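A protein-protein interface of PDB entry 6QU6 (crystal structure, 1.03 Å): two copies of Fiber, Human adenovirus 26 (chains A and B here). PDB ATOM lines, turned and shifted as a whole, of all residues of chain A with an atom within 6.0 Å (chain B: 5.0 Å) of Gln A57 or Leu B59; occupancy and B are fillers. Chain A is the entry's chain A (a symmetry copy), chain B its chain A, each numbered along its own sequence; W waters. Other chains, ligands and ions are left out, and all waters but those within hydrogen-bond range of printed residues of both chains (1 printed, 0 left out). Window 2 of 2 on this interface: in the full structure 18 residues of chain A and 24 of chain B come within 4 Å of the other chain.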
ATOM      1  N   THR A  52       6.879 -12.529 -10.293  1.00  0.00           N
ATOM      2  CA  THR A  52       6.956 -11.855 -11.590  1.00  0.00           C
ATOM      3  C   THR A  52       8.401 -11.467 -11.854  1.00  0.00           C
ATOM      4  O   THR A  52       9.038 -10.836 -11.026  1.00  0.00           O
ATOM      5  CB  THR A  52       6.027 -10.655 -11.596  1.00  0.00           C
ATOM      6  OG1 THR A  52       4.700 -11.080 -11.291  1.00  0.00           O
ATOM      7  CG2 THR A  52       6.113  -9.925 -12.908  1.00  0.00           C
ATOM      8  N   LYS A  53       8.897 -11.887 -12.996  1.00  0.00           N
ATOM      9  CA  LYS A  53      10.289 -11.620 -13.365  1.00  0.00           C
ATOM     10  C   LYS A  53      10.406 -10.185 -13.839  1.00  0.00           C
ATOM     11  O   LYS A  53       9.743  -9.822 -14.804  1.00  0.00           O
ATOM     12  CB  LYS A  53      10.675 -12.617 -14.447  1.00  0.00           C
ATOM     13  CG  LYS A  53      11.988 -12.344 -15.132  1.00  0.00           C
ATOM     14  CD  LYS A  53      13.092 -12.874 -14.335  1.00  0.00           C
ATOM     15  CE  LYS A  53      14.314 -13.131 -15.171  1.00  0.00           C
ATOM     16  NZ  LYS A  53      15.454 -13.316 -14.263  1.00  0.00           N
ATOM     17  N   CYS A  54      11.324  -9.441 -13.227  1.00  0.00           N
ATOM     18  CA  CYS A  54      11.662  -8.040 -13.557  1.00  0.00           C
ATOM     19  C   CYS A  54      13.184  -7.954 -13.757  1.00  0.00           C
ATOM     20  O   CYS A  54      13.854  -7.423 -12.860  1.00  0.00           O
ATOM     21  CB  CYS A  54      11.185  -7.114 -12.441  1.00  0.00           C
ATOM     22  SG  CYS A  54       9.428  -7.273 -12.005  1.00  0.00           S
ATOM     23  N   GLY A  55      13.703  -8.513 -14.859  1.00  0.00           N
ATOM     24  CA  GLY A  55      15.148  -8.596 -15.133  1.00  0.00           C
ATOM     25  C   GLY A  55      15.830  -9.440 -14.073  1.00  0.00           C
ATOM     26  O   GLY A  55      15.423 -10.577 -13.832  1.00  0.00           O
ATOM     27  N   SER A  56      16.807  -8.832 -13.405  1.00  0.00           N
ATOM     28  CA  SER A  56      17.706  -9.459 -12.409  1.00  0.00           C
ATOM     29  C   SER A  56      16.933  -9.878 -11.156  1.00  0.00           C
ATOM     30  O   SER A  56      17.459 -10.711 -10.402  1.00  0.00           O
ATOM     31  CB  SER A  56      18.817  -8.495 -12.087  1.00  0.00           C
ATOM     32  OG  SER A  56      18.286  -7.194 -11.864  1.00  0.00           O
ATOM     33  N   GLN A  57      15.741  -9.313 -10.929  1.00  0.00           N
ATOM     34  CA  GLN A  57      14.977  -9.582  -9.697  1.00  0.00           C
ATOM     35  C   GLN A  57      13.621 -10.179 -10.039  1.00  0.00           C
ATOM     36  O   GLN A  57      13.073  -9.969 -11.120  1.00  0.00           O
ATOM     37  CB  GLN A  57      14.773  -8.337  -8.842  1.00  0.00           C
ATOM     38  CG  GLN A  57      16.042  -7.851  -8.185  1.00  0.00           C
ATOM     39  CD  GLN A  57      15.785  -6.624  -7.340  1.00  0.00           C
ATOM     40  OE1 GLN A  57      15.155  -6.684  -6.280  1.00  0.00           O
ATOM     41  NE2 GLN A  57      16.255  -5.483  -7.823  1.00  0.00           N
ATOM     42  N   VAL A  58      13.126 -10.938  -9.098  1.00  0.00           N
ATOM     43  CA  VAL A  58      11.705 -11.315  -9.068  1.00  0.00           C
ATOM     44  C   VAL A  58      11.017 -10.412  -8.055  1.00  0.00           C
ATOM     45  O   VAL A  58      11.536 -10.184  -6.957  1.00  0.00           O
ATOM     46  CB  VAL A  58      11.538 -12.795  -8.700  1.00  0.00           C
ATOM     47  CG1 VAL A  58      10.168 -13.093  -8.111  1.00  0.00           C
ATOM     48  CG2 VAL A  58      11.772 -13.651  -9.933  1.00  0.00           C
ATOM     49  N   LEU A  59       9.841  -9.931  -8.429  1.00  0.00           N
ATOM     50  CA  LEU A  59       8.879  -9.257  -7.547  1.00  0.00           C
ATOM     51  C   LEU A  59       7.861 -10.306  -7.097  1.00  0.00           C
ATOM     52  O   LEU A  59       7.162 -10.893  -7.924  1.00  0.00           O
ATOM     53  CB  LEU A  59       8.231  -8.126  -8.329  1.00  0.00           C
ATOM     54  CG  LEU A  59       7.214  -7.296  -7.567  1.00  0.00           C
ATOM     55  CD1 LEU A  59       7.859  -6.562  -6.392  1.00  0.00           C
ATOM     56  CD2 LEU A  59       6.528  -6.319  -8.516  1.00  0.00           C
ATOM     57  N   PHE A 201       7.741  -8.582  -1.779  1.00  0.00           N
ATOM     58  CA  PHE A 201       9.178  -8.774  -1.569  1.00  0.00           C
ATOM     59  C   PHE A 201       9.861  -8.886  -2.920  1.00  0.00           C
ATOM     60  O   PHE A 201       9.199  -9.007  -3.948  1.00  0.00           O
ATOM     61  CB  PHE A 201       9.419  -9.998  -0.690  1.00  0.00           C
ATOM     62  CG  PHE A 201       8.977 -11.299  -1.289  1.00  0.00           C
ATOM     63  CD1 PHE A 201       7.656 -11.724  -1.215  1.00  0.00           C
ATOM     64  CD2 PHE A 201       9.892 -12.142  -1.900  1.00  0.00           C
ATOM     65  CE1 PHE A 201       7.251 -12.928  -1.783  1.00  0.00           C
ATOM     66  CE2 PHE A 201       9.496 -13.357  -2.449  1.00  0.00           C
ATOM     67  CZ  PHE A 201       8.181 -13.754  -2.376  1.00  0.00           C
ATOM     68  N   SER A 202      11.182  -8.894  -2.918  1.00  0.00           N
ATOM     69  CA  SER A 202      11.937  -9.177  -4.141  1.00  0.00           C
ATOM     70  C   SER A 202      13.165  -9.978  -3.778  1.00  0.00           C
ATOM     71  O   SER A 202      13.587 -10.011  -2.611  1.00  0.00           O
ATOM     72  CB  SER A 202      12.298  -7.929  -4.901  1.00  0.00           C
ATOM     73  OG  SER A 202      13.366  -7.234  -4.284  1.00  0.00           O
ATOM     74  N   TYR A 203      13.782 -10.565  -4.784  1.00  0.00           N
ATOM     75  CA  TYR A 203      15.056 -11.273  -4.606  1.00  0.00           C
ATOM     76  C   TYR A 203      15.781 -11.310  -5.932  1.00  0.00           C
ATOM     77  O   TYR A 203      15.165 -11.237  -7.018  1.00  0.00           O
ATOM     78  CB  TYR A 203      14.851 -12.676  -4.029  1.00  0.00           C
ATOM     79  CG  TYR A 203      14.007 -13.602  -4.874  1.00  0.00           C
ATOM     80  CD1 TYR A 203      14.551 -14.411  -5.854  1.00  0.00           C
ATOM     81  CD2 TYR A 203      12.644 -13.692  -4.678  1.00  0.00           C
ATOM     82  CE1 TYR A 203      13.781 -15.279  -6.613  1.00  0.00           C
ATOM     83  CE2 TYR A 203      11.845 -14.539  -5.426  1.00  0.00           C
ATOM     84  CZ  TYR A 203      12.415 -15.343  -6.395  1.00  0.00           C
ATOM     85  OH  TYR A 203      11.605 -16.163  -7.124  1.00  0.00           O
ATOM     86  N   LEU A 204      17.106 -11.419  -5.859  1.00  0.00           N
ATOM     87  CA  LEU A 204      17.960 -11.524  -7.062  1.00  0.00           C
ATOM     88  C   LEU A 204      17.852 -12.931  -7.632  1.00  0.00           C
ATOM     89  O   LEU A 204      17.853 -13.899  -6.866  1.00  0.00           O
ATOM     90  CB  LEU A 204      19.421 -11.242  -6.715  1.00  0.00           C
ATOM     91  CG  LEU A 204      20.369 -11.161  -7.912  1.00  0.00           C
ATOM     92  CD1 LEU A 204      20.169  -9.848  -8.674  1.00  0.00           C
ATOM     93  CD2 LEU A 204      21.809 -11.310  -7.451  1.00  0.00           C
ATOM     94  N   THR A 205      17.829 -13.025  -8.954  1.00  0.00           N
ATOM     95  CA  THR A 205      17.599 -14.291  -9.665  1.00  0.00           C
ATOM     96  C   THR A 205      18.913 -14.902 -10.143  1.00  0.00           C
ATOM     97  O   THR A 205      19.911 -14.188 -10.333  1.00  0.00           O
ATOM     98  CB  THR A 205      16.672 -14.070 -10.858  1.00  0.00           C
ATOM     99  OG1 THR A 205      15.374 -13.716 -10.373  1.00  0.00           O
ATOM    100  CG2 THR A 205      16.594 -15.295 -11.731  1.00  0.00           C
ATOM    101  N   THR B  50      21.287  -4.069  -5.191  1.00  0.00           N
ATOM    102  CA  THR B  50      20.860  -4.264  -6.583  1.00  0.00           C
ATOM    103  C   THR B  50      19.749  -3.266  -6.870  1.00  0.00           C
ATOM    104  O   THR B  50      18.805  -3.169  -6.086  1.00  0.00           O
ATOM    105  CB  THR B  50      20.362  -5.688  -6.758  1.00  0.00           C
ATOM    106  OG1 THR B  50      21.376  -6.592  -6.320  1.00  0.00           O
ATOM    107  CG2 THR B  50      19.935  -5.960  -8.175  1.00  0.00           C
ATOM    108  N   LEU B  51      19.898  -2.555  -7.978  1.00  0.00           N
ATOM    109  CA  LEU B  51      18.901  -1.590  -8.478  1.00  0.00           C
ATOM    110  C   LEU B  51      18.475  -2.087  -9.854  1.00  0.00           C
ATOM    111  O   LEU B  51      19.299  -2.114 -10.775  1.00  0.00           O
ATOM    112  CB  LEU B  51      19.518  -0.201  -8.565  1.00  0.00           C
ATOM    113  CG  LEU B  51      20.081   0.373  -7.271  1.00  0.00           C
ATOM    114  CD1 LEU B  51      20.683   1.741  -7.511  1.00  0.00           C
ATOM    115  CD2 LEU B  51      19.047   0.437  -6.155  1.00  0.00           C
ATOM    116  N   THR B  52      17.201  -2.460 -10.005  1.00  0.00           N
ATOM    117  CA  THR B  52      16.678  -2.943 -11.284  1.00  0.00           C
ATOM    118  C   THR B  52      15.655  -1.946 -11.801  1.00  0.00           C
ATOM    119  O   THR B  52      14.732  -1.577 -11.093  1.00  0.00           O
ATOM    120  CB  THR B  52      16.090  -4.330 -11.102  1.00  0.00           C
ATOM    121  OG1 THR B  52      17.084  -5.201 -10.567  1.00  0.00           O
ATOM    122  CG2 THR B  52      15.515  -4.834 -12.397  1.00  0.00           C
ATOM    123  N   CYS B  54      12.572  -0.681 -13.651  1.00  0.00           N
ATOM    124  CA  CYS B  54      11.215  -1.139 -14.016  1.00  0.00           C
ATOM    125  C   CYS B  54      10.412   0.083 -14.490  1.00  0.00           C
ATOM    126  O   CYS B  54       9.554   0.541 -13.722  1.00  0.00           O
ATOM    127  CB  CYS B  54      10.557  -1.819 -12.818  1.00  0.00           C
ATOM    128  SG  CYS B  54      11.521  -3.167 -12.072  1.00  0.00           S
ATOM    129  N   GLN B  57      10.125   3.406 -12.195  1.00  0.00           N
ATOM    130  CA  GLN B  57      10.637   3.091 -10.849  1.00  0.00           C
ATOM    131  C   GLN B  57      11.845   2.172 -10.948  1.00  0.00           C
ATOM    132  O   GLN B  57      12.013   1.422 -11.907  1.00  0.00           O
ATOM    133  CB  GLN B  57       9.589   2.443  -9.952  1.00  0.00           C
ATOM    134  CG  GLN B  57       8.496   3.394  -9.530  1.00  0.00           C
ATOM    135  CD  GLN B  57       7.489   2.708  -8.635  1.00  0.00           C
ATOM    136  OE1 GLN B  57       7.768   2.376  -7.478  1.00  0.00           O
ATOM    137  NE2 GLN B  57       6.306   2.464  -9.177  1.00  0.00           N
ATOM    138  N   VAL B  58      12.674   2.281  -9.943  1.00  0.00           N
ATOM    139  CA  VAL B  58      13.693   1.260  -9.661  1.00  0.00           C
ATOM    140  C   VAL B  58      13.167   0.394  -8.526  1.00  0.00           C
ATOM    141  O   VAL B  58      12.631   0.907  -7.537  1.00  0.00           O
ATOM    142  CB  VAL B  58      15.033   1.911  -9.292  1.00  0.00           C
ATOM    143  CG1 VAL B  58      15.916   0.986  -8.467  1.00  0.00           C
ATOM    144  CG2 VAL B  58      15.757   2.329 -10.560  1.00  0.00           C
ATOM    145  N   LEU B  59      13.352  -0.909  -8.671  1.00  0.00           N
ATOM    146  CA  LEU B  59      13.168  -1.916  -7.620  1.00  0.00           C
ATOM    147  C   LEU B  59      14.543  -2.192  -7.008  1.00  0.00           C
ATOM    148  O   LEU B  59      15.459  -2.635  -7.702  1.00  0.00           O
ATOM    149  CB  LEU B  59      12.563  -3.158  -8.253  1.00  0.00           C
ATOM    150  CG  LEU B  59      12.280  -4.310  -7.306  1.00  0.00           C
ATOM    151  CD1 LEU B  59      11.236  -3.929  -6.258  1.00  0.00           C
ATOM    152  CD2 LEU B  59      11.839  -5.536  -8.100  1.00  0.00           C
ATOM    153  N   GLY B  60      14.681  -1.876  -5.736  1.00  0.00           N
ATOM    154  CA  GLY B  60      15.935  -1.998  -5.021  1.00  0.00           C
ATOM    155  C   GLY B  60      15.904  -3.092  -3.994  1.00  0.00           C
ATOM    156  O   GLY B  60      14.849  -3.414  -3.425  1.00  0.00           O
ATOM    157  N   ASN B  61      17.087  -3.568  -3.669  1.00  0.00           N
ATOM    158  CA  ASN B  61      17.245  -4.671  -2.725  1.00  0.00           C
ATOM    159  C   ASN B  61      18.587  -4.458  -2.045  1.00  0.00           C
ATOM    160  O   ASN B  61      19.581  -4.265  -2.758  1.00  0.00           O
ATOM    161  CB  ASN B  61      17.118  -5.966  -3.508  1.00  0.00           C
ATOM    162  CG  ASN B  61      17.192  -7.140  -2.597  1.00  0.00           C
ATOM    163  OD1 ASN B  61      16.161  -7.647  -2.174  1.00  0.00           O
ATOM    164  ND2 ASN B  61      18.387  -7.525  -2.220  1.00  0.00           N
ATOM    165  N   THR B 200      13.633  -4.798   0.574  1.00  0.00           N
ATOM    166  CA  THR B 200      13.081  -4.450  -0.752  1.00  0.00           C
ATOM    167  C   THR B 200      12.507  -3.042  -0.679  1.00  0.00           C
ATOM    168  O   THR B 200      11.867  -2.688   0.318  1.00  0.00           O
ATOM    169  CB  THR B 200      12.050  -5.481  -1.242  1.00  0.00           C
ATOM    170  OG1 THR B 200      12.814  -6.682  -1.477  1.00  0.00           O
ATOM    171  CG2 THR B 200      11.400  -5.138  -2.574  1.00  0.00           C
ATOM    172  N   PHE B 201      12.694  -2.265  -1.731  1.00  0.00           N
ATOM    173  CA  PHE B 201      12.142  -0.910  -1.789  1.00  0.00           C
ATOM    174  C   PHE B 201      12.010  -0.495  -3.244  1.00  0.00           C
ATOM    175  O   PHE B 201      12.518  -1.171  -4.136  1.00  0.00           O
ATOM    176  CB  PHE B 201      13.020   0.046  -0.988  1.00  0.00           C
ATOM    177  CG  PHE B 201      14.414   0.214  -1.515  1.00  0.00           C
ATOM    178  CD1 PHE B 201      15.421  -0.691  -1.210  1.00  0.00           C
ATOM    179  CD2 PHE B 201      14.745   1.310  -2.297  1.00  0.00           C
ATOM    180  CE1 PHE B 201      16.710  -0.535  -1.712  1.00  0.00           C
ATOM    181  CE2 PHE B 201      16.037   1.482  -2.782  1.00  0.00           C
ATOM    182  CZ  PHE B 201      17.019   0.568  -2.477  1.00  0.00           C
ATOM    183  N   SER B 202      11.371   0.636  -3.483  1.00  0.00           N
ATOM    184  CA  SER B 202      11.343   1.218  -4.827  1.00  0.00           C
ATOM    185  C   SER B 202      11.410   2.722  -4.706  1.00  0.00           C
ATOM    186  O   SER B 202      11.143   3.291  -3.636  1.00  0.00           O
ATOM    187  CB  SER B 202      10.140   0.783  -5.620  1.00  0.00           C
ATOM    188  OG  SER B 202       8.967   1.452  -5.198  1.00  0.00           O
HETATM  189  O   HOH W   1      15.648 -10.123  -0.758  1.00  0.00           O
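The side-chain amide nitrogen of Gln A57 is in hydrogen-bond range of the backbone carbonyl oxygen of Leu B59, 3.0 Å away.
The side-chain hydroxyl (OG) of Ser A56 sits at hydrogen-bond distance from the side-chain hydroxyl (OG1) of Thr B52 (2.7 Å).
The side-chain hydroxyl of Thr B200 sits at hydrogen-bond distance from the side-chain hydroxyl of Ser A202, 2.9 Å away.
OG1 of Thr B52 lies within hydrogen-bond range of NE2 of Gln A57, 2.9 Å away.
The backbone NH (N) of Thr A205 lies within hydrogen-bond range of the backbone carbonyl oxygen (O) of Ser A56, 2.8 Å away.
The backbone NH (N) of Thr B50 is in hydrogen-bond range of the backbone carbonyl oxygen (O) of Asn B61 (3.0 Å).
The backbone carbonyl oxygen (O) of Thr B52 lies within hydrogen-bond range of the side-chain sulfur (SG) of Cys B54, at 3.7 Å.
O of Thr B52 is in hydrogen-bond range of N of Leu B59.
The side-chain sulfur (SG) of Cys A54 lies within hydrogen-bond range of the backbone carbonyl oxygen (O) of Thr A52, 3.7 Å away.
The side-chain amide oxygen (OE1) of Gln A57 is in hydrogen-bond range of the side-chain hydroxyl (OG) of Ser A202 (2.7 Å).
Thr B52 touches Cys A54.
SG of Cys B54 touches CB of Cys A54, 3.98 Å away.
Thr B50 touches Gln A57.
Gln A57 touches Asn B61 (OE1 to CB, 3.5 Å).
Phe A201 touches Thr B200 (C to OG1, 3.96 Å).
OD1 of Asn B61 touches O of Ser A202, 3.5 Å away.
Leu A204 touches Thr B50 (CD1 to CG2, 3.9 Å).
Of the printed residues of chain B, Cys A54 touches Thr B52 and Cys B54.
Of the printed residues of chain B, Ser A56 touches Thr B52.
Of the printed residues of chain B, Gln A57 touches Thr B50, Thr B52, Leu B59 and Asn B61.
Of the printed residues of chain A, Cys B54 touches Cys A54 (3.98 Å).
Val B58 touches none of the printed residues of chain A.
Leu B59 touches just one residue of chain A: Gln A57 (3.0 Å).
The nearest residue of chain A that does not touch Leu B59 is Ser A202 (4.02 Å).
The nearest printed residue of chain A that does not touch Thr B200 is Tyr A203 (5.2 Å).
Of the 12 printed residues of chain B, 6 touch a printed residue of chain A.
Printed residues of chain B that touch a printed residue of chain A: Thr B50, Thr B52, Cys B54, Leu B59, Asn B61 and Thr B200.
Along chain B the printed residues that touch a printed residue of chain A span positions 50 to 200.
Cys A54 touches Thr B52, but with the chains exchanged Thr A52 does not touch Cys B54 (8.1 Å).
Cys A54 touches its own counterpart, Cys B54.
Gln A57 touches Thr B52, but with the chains exchanged Thr A52 does not touch Gln B57 (12.6 Å).
Gln A57 touches Leu B59, but with the chains exchanged Leu A59 does not touch Gln B57 (8.8 Å).
Of the 11 pairs that touch across the chains among the printed residues, 1 has its exchanged pair printed and touching as well.
Water W1 lies within hydrogen-bond range of O of Ser A202 (2.8 Å) and OD1 of Asn B61 (2.9 Å).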
